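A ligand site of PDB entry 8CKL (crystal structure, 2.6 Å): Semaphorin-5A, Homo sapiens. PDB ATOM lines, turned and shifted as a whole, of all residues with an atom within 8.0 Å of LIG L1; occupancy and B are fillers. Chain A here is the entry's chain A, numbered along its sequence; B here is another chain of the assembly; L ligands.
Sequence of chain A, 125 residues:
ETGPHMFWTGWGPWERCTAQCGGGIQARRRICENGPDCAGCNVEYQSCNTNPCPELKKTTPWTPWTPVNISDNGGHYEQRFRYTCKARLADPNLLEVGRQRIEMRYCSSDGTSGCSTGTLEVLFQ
The backbone NH (N) of Trp 8 sits close to an oxygen (O1) of LIG L1 (3.3 Å). The aromatic ring (CD1) of Trp 8 is covalently linked to a carbon (C1) of LIG L1 (1.5 Å). An oxygen (O3) of LIG L1 lies within hydrogen-bond range of the backbone carbonyl oxygen (O) of Ala 39. The guanidinium group (NH1) of Arg 30 is in hydrogen-bond range of an oxygen (O5) of LIG L1 (3.0 Å). N of Trp 11 lies close to O1 of LG2 L2 (3.2 Å). A carbon (C1) of LG2 L2 is covalently linked to the aromatic ring (CD1) of Trp 11.
Phe 7 touches LIG L1 (CA to O1, 3.9 Å). Hydrophobic or aromatic side chains within 4 Å of LIG L1: Trp 8 and Ala 39.
The backbone carbonyl oxygen (O) of Ala 39 lies within hydrogen-bond range of the indole nitrogen (NE1) of Trp 8, at 2.4 Å. The backbone carbonyl oxygen (O) of Cys 41 lies within hydrogen-bond range of the guanidinium group (NE) of Arg 30 (2.6 Å). O of Phe 7 is in hydrogen-bond range of N of Glu 33, at 3.4 Å. The side-chain sulfur (SG) of Cys 38 of chain A is disulfide-bonded to the side-chain sulfur (SG) of Cys 32 (2.0 Å).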
ATOM      1  N   MET A   6       7.326  21.567 -16.567  1.00  0.00           N
ATOM      2  CA  MET A   6       7.579  21.028 -17.899  1.00  0.00           C
ATOM      3  C   MET A   6       6.277  20.839 -18.669  1.00  0.00           C
ATOM      4  O   MET A   6       5.349  20.169 -18.209  1.00  0.00           O
ATOM      5  CB  MET A   6       8.336  19.698 -17.806  1.00  0.00           C
ATOM      6  CG  MET A   6       9.729  19.833 -17.216  1.00  0.00           C
ATOM      7  SD  MET A   6      10.584  18.261 -17.050  1.00  0.00           S
ATOM      8  CE  MET A   6       9.504  17.410 -15.905  1.00  0.00           C
ATOM      9  N   PHE A   7       6.202  21.437 -19.856  1.00  0.00           N
ATOM     10  CA  PHE A   7       5.011  21.388 -20.684  1.00  0.00           C
ATOM     11  C   PHE A   7       5.414  21.430 -22.151  1.00  0.00           C
ATOM     12  O   PHE A   7       6.399  22.082 -22.517  1.00  0.00           O
ATOM     13  CB  PHE A   7       4.041  22.539 -20.364  1.00  0.00           C
ATOM     14  CG  PHE A   7       4.624  23.905 -20.557  1.00  0.00           C
ATOM     15  CD1 PHE A   7       4.476  24.572 -21.761  1.00  0.00           C
ATOM     16  CD2 PHE A   7       5.329  24.529 -19.541  1.00  0.00           C
ATOM     17  CE1 PHE A   7       5.011  25.834 -21.943  1.00  0.00           C
ATOM     18  CE2 PHE A   7       5.868  25.797 -19.716  1.00  0.00           C
ATOM     19  CZ  PHE A   7       5.704  26.441 -20.921  1.00  0.00           C
ATOM     20  N   TRP A   8       4.653  20.734 -22.986  1.00  0.00           N
ATOM     21  CA  TRP A   8       4.900  20.693 -24.419  1.00  0.00           C
ATOM     22  C   TRP A   8       4.201  21.862 -25.099  1.00  0.00           C
ATOM     23  O   TRP A   8       3.006  22.080 -24.876  1.00  0.00           O
ATOM     24  CB  TRP A   8       4.410  19.381 -25.028  1.00  0.00           C
ATOM     25  CG  TRP A   8       5.349  18.227 -24.946  1.00  0.00           C
ATOM     26  CD1 TRP A   8       5.146  17.051 -24.287  1.00  0.00           C
ATOM     27  CD2 TRP A   8       6.631  18.111 -25.581  1.00  0.00           C
ATOM     28  NE1 TRP A   8       6.232  16.219 -24.464  1.00  0.00           N
ATOM     29  CE2 TRP A   8       7.156  16.845 -25.257  1.00  0.00           C
ATOM     30  CE3 TRP A   8       7.397  18.966 -26.394  1.00  0.00           C
ATOM     31  CZ2 TRP A   8       8.396  16.415 -25.706  1.00  0.00           C
ATOM     32  CZ3 TRP A   8       8.622  18.530 -26.844  1.00  0.00           C
ATOM     33  CH2 TRP A   8       9.121  17.264 -26.493  1.00  0.00           C
ATOM     34  N   THR A   9       4.941  22.589 -25.921  1.00  0.00           N
ATOM     35  CA  THR A   9       4.347  23.657 -26.710  1.00  0.00           C
ATOM     36  C   THR A   9       3.546  23.062 -27.864  1.00  0.00           C
ATOM     37  O   THR A   9       3.625  21.870 -28.169  1.00  0.00           O
ATOM     38  CB  THR A   9       5.421  24.606 -27.231  1.00  0.00           C
ATOM     39  OG1 THR A   9       6.371  23.875 -28.022  1.00  0.00           O
ATOM     40  CG2 THR A   9       6.151  25.275 -26.072  1.00  0.00           C
ATOM     41  N   GLY A  10       2.764  23.917 -28.515  1.00  0.00           N
ATOM     42  CA  GLY A  10       1.989  23.467 -29.660  1.00  0.00           C
ATOM     43  C   GLY A  10       2.866  23.050 -30.813  1.00  0.00           C
ATOM     44  O   GLY A  10       3.984  23.535 -30.989  1.00  0.00           O
ATOM     45  N   TRP A  11       2.356  22.121 -31.617  1.00  0.00           N
ATOM     46  CA  TRP A  11       3.099  21.633 -32.769  1.00  0.00           C
ATOM     47  C   TRP A  11       3.277  22.771 -33.769  1.00  0.00           C
ATOM     48  O   TRP A  11       2.337  23.523 -34.068  1.00  0.00           O
ATOM     49  CB  TRP A  11       2.376  20.457 -33.423  1.00  0.00           C
ATOM     50  CG  TRP A  11       2.514  19.165 -32.693  1.00  0.00           C
ATOM     51  CD1 TRP A  11       1.560  18.527 -31.957  1.00  0.00           C
ATOM     52  CD2 TRP A  11       3.679  18.320 -32.640  1.00  0.00           C
ATOM     53  NE1 TRP A  11       2.055  17.351 -31.443  1.00  0.00           N
ATOM     54  CE2 TRP A  11       3.354  17.205 -31.844  1.00  0.00           C
ATOM     55  CE3 TRP A  11       4.966  18.411 -33.181  1.00  0.00           C
ATOM     56  CZ2 TRP A  11       4.259  16.187 -31.578  1.00  0.00           C
ATOM     57  CZ3 TRP A  11       5.862  17.399 -32.915  1.00  0.00           C
ATOM     58  CH2 TRP A  11       5.513  16.301 -32.121  1.00  0.00           C
ATOM     59  N   ARG A  30       8.233  20.569 -31.882  1.00  0.00           N
ATOM     60  CA  ARG A  30       7.707  21.215 -30.690  1.00  0.00           C
ATOM     61  C   ARG A  30       8.832  21.250 -29.667  1.00  0.00           C
ATOM     62  O   ARG A  30       9.807  20.507 -29.764  1.00  0.00           O
ATOM     63  CB  ARG A  30       6.465  20.500 -30.146  1.00  0.00           C
ATOM     64  CG  ARG A  30       6.660  19.039 -29.804  1.00  0.00           C
ATOM     65  CD  ARG A  30       5.401  18.462 -29.181  1.00  0.00           C
ATOM     66  NE  ARG A  30       5.562  17.080 -28.748  1.00  0.00           N
ATOM     67  CZ  ARG A  30       4.614  16.352 -28.191  1.00  0.00           C
ATOM     68  NH1 ARG A  30       3.399  16.842 -27.966  1.00  0.00           N
ATOM     69  NH2 ARG A  30       4.875  15.093 -27.837  1.00  0.00           N
ATOM     70  N   ILE A  31       8.684  22.116 -28.661  1.00  0.00           N
ATOM     71  CA  ILE A  31       9.752  22.382 -27.709  1.00  0.00           C
ATOM     72  C   ILE A  31       9.316  21.988 -26.304  1.00  0.00           C
ATOM     73  O   ILE A  31       8.223  22.350 -25.862  1.00  0.00           O
ATOM     74  CB  ILE A  31      10.179  23.866 -27.739  1.00  0.00           C
ATOM     75  N   CYS A  32      10.176  21.231 -25.620  1.00  0.00           N
ATOM     76  CA  CYS A  32       9.984  20.910 -24.216  1.00  0.00           C
ATOM     77  C   CYS A  32      10.526  22.047 -23.358  1.00  0.00           C
ATOM     78  O   CYS A  32      11.674  22.486 -23.556  1.00  0.00           O
ATOM     79  CB  CYS A  32      10.677  19.588 -23.878  1.00  0.00           C
ATOM     80  SG  CYS A  32      10.800  19.181 -22.113  1.00  0.00           S
ATOM     81  N   GLU A  33       9.728  22.530 -22.421  1.00  0.00           N
ATOM     82  CA  GLU A  33      10.081  23.706 -21.636  1.00  0.00           C
ATOM     83  C   GLU A  33      10.560  23.319 -20.244  1.00  0.00           C
ATOM     84  O   GLU A  33       9.969  22.462 -19.586  1.00  0.00           O
ATOM     85  CB  GLU A  33       8.886  24.659 -21.527  1.00  0.00           C
ATOM     86  N   ASP A  37      13.706  16.115 -20.280  1.00  0.00           N
ATOM     87  CA  ASP A  37      12.977  14.853 -20.426  1.00  0.00           C
ATOM     88  C   ASP A  37      11.480  15.121 -20.309  1.00  0.00           C
ATOM     89  O   ASP A  37      10.907  15.074 -19.217  1.00  0.00           O
ATOM     90  CB  ASP A  37      13.440  13.840 -19.380  1.00  0.00           C
ATOM     91  CG  ASP A  37      14.848  13.347 -19.631  1.00  0.00           C
ATOM     92  OD1 ASP A  37      15.248  13.242 -20.817  1.00  0.00           O
ATOM     93  OD2 ASP A  37      15.566  13.053 -18.652  1.00  0.00           O
ATOM     94  N   CYS A  38      10.847  15.405 -21.447  1.00  0.00           N
ATOM     95  CA  CYS A  38       9.398  15.554 -21.534  1.00  0.00           C
ATOM     96  C   CYS A  38       8.779  14.286 -22.099  1.00  0.00           C
ATOM     97  O   CYS A  38       9.404  13.545 -22.856  1.00  0.00           O
ATOM     98  CB  CYS A  38       9.015  16.746 -22.418  1.00  0.00           C
ATOM     99  SG  CYS A  38       8.994  18.385 -21.646  1.00  0.00           S
ATOM    100  N   ALA A  39       7.526  14.040 -21.714  1.00  0.00           N
ATOM    101  CA  ALA A  39       6.796  12.880 -22.212  1.00  0.00           C
ATOM    102  C   ALA A  39       6.230  13.214 -23.587  1.00  0.00           C
ATOM    103  O   ALA A  39       5.350  14.064 -23.719  1.00  0.00           O
ATOM    104  CB  ALA A  39       5.685  12.487 -21.248  1.00  0.00           C
ATOM    105  N   GLY A  40       6.741  12.538 -24.624  1.00  0.00           N
ATOM    106  CA  GLY A  40       6.373  12.770 -26.006  1.00  0.00           C
ATOM    107  C   GLY A  40       7.620  12.945 -26.838  1.00  0.00           C
ATOM    108  O   GLY A  40       8.725  12.581 -26.422  1.00  0.00           O
ATOM    109  N   CYS A  41       7.460  13.508 -28.036  1.00  0.00           N
ATOM    110  CA  CYS A  41       8.575  13.664 -28.953  1.00  0.00           C
ATOM    111  C   CYS A  41       8.648  15.079 -29.502  1.00  0.00           C
ATOM    112  O   CYS A  41       7.616  15.719 -29.721  1.00  0.00           O
ATOM    113  CB  CYS A  41       8.470  12.651 -30.100  1.00  0.00           C
ATOM    114  SG  CYS A  41       8.953  11.041 -29.484  1.00  0.00           S
ATOM    115  N   PRO B  36       3.187   4.046 -19.308  1.00  0.00           N
ATOM    116  CA  PRO B  36       2.675   4.788 -20.457  1.00  0.00           C
ATOM    117  C   PRO B  36       3.380   6.117 -20.694  1.00  0.00           C
ATOM    118  O   PRO B  36       3.130   6.752 -21.726  1.00  0.00           O
ATOM    119  CB  PRO B  36       1.207   5.025 -20.070  1.00  0.00           C
ATOM    120  CG  PRO B  36       1.266   5.180 -18.579  1.00  0.00           C
ATOM    121  CD  PRO B  36       2.379   4.284 -18.090  1.00  0.00           C
ATOM    122  N   ASP B  37       4.247   6.547 -19.772  1.00  0.00           N
ATOM    123  CA  ASP B  37       4.941   7.834 -19.862  1.00  0.00           C
ATOM    124  C   ASP B  37       6.427   7.608 -19.568  1.00  0.00           C
ATOM    125  O   ASP B  37       6.850   7.673 -18.408  1.00  0.00           O
ATOM    126  CB  ASP B  37       4.320   8.856 -18.918  1.00  0.00           C
ATOM    127  N   CYS B  38       7.202   7.351 -20.604  1.00  0.00           N
ATOM    128  CA  CYS B  38       8.649   7.254 -20.488  1.00  0.00           C
ATOM    129  C   CYS B  38       9.297   8.560 -20.912  1.00  0.00           C
ATOM    130  O   CYS B  38       8.780   9.277 -21.779  1.00  0.00           O
ATOM    131  CB  CYS B  38       9.206   6.109 -21.344  1.00  0.00           C
ATOM    132  SG  CYS B  38       9.198   4.445 -20.617  1.00  0.00           S
HETATM  133  C1  LIG L   1       3.713  16.879 -23.924  1.00  0.00           C
HETATM  134  C2  LIG L   1       3.753  16.583 -22.424  1.00  0.00           C
HETATM  135  C3  LIG L   1       2.378  16.184 -21.925  1.00  0.00           C
HETATM  136  C4  LIG L   1       1.786  15.064 -22.771  1.00  0.00           C
HETATM  137  C5  LIG L   1       1.876  15.373 -24.264  1.00  0.00           C
HETATM  138  C6  LIG L   1       0.967  16.497 -24.720  1.00  0.00           C
HETATM  139  O1  LIG L   1       4.220  17.726 -21.726  1.00  0.00           O
HETATM  140  O2  LIG L   1       1.507  17.321 -21.877  1.00  0.00           O
HETATM  141  O3  LIG L   1       2.464  13.841 -22.503  1.00  0.00           O
HETATM  142  O4  LIG L   1       3.221  15.735 -24.623  1.00  0.00           O
HETATM  143  O5  LIG L   1       1.099  16.730 -26.121  1.00  0.00           O
HETATM  144  C1  LG2 L   2       0.133  18.788 -31.582  1.00  0.00           C
HETATM  145  C2  LG2 L   2      -0.070  19.002 -30.089  1.00  0.00           C
HETATM  146  C3  LG2 L   2      -1.557  19.031 -29.762  1.00  0.00           C
HETATM  147  C4  LG2 L   2      -2.271  17.803 -30.323  1.00  0.00           C
HETATM  148  C5  LG2 L   2      -1.921  17.572 -31.796  1.00  0.00           C
HETATM  149  C6  LG2 L   2      -2.496  18.607 -32.733  1.00  0.00           C
HETATM  150  O1  LG2 L   2       0.542  20.231 -29.695  1.00  0.00           O
HETATM  151  O2  LG2 L   2      -2.152  20.240 -30.224  1.00  0.00           O
HETATM  152  O3  LG2 L   2      -1.907  16.646 -29.567  1.00  0.00           O
HETATM  153  O4  LG2 L   2      -0.494  17.570 -31.977  1.00  0.00           O
HETATM  154  O5  LG2 L   2      -2.131  18.335 -34.085  1.00  0.00           O
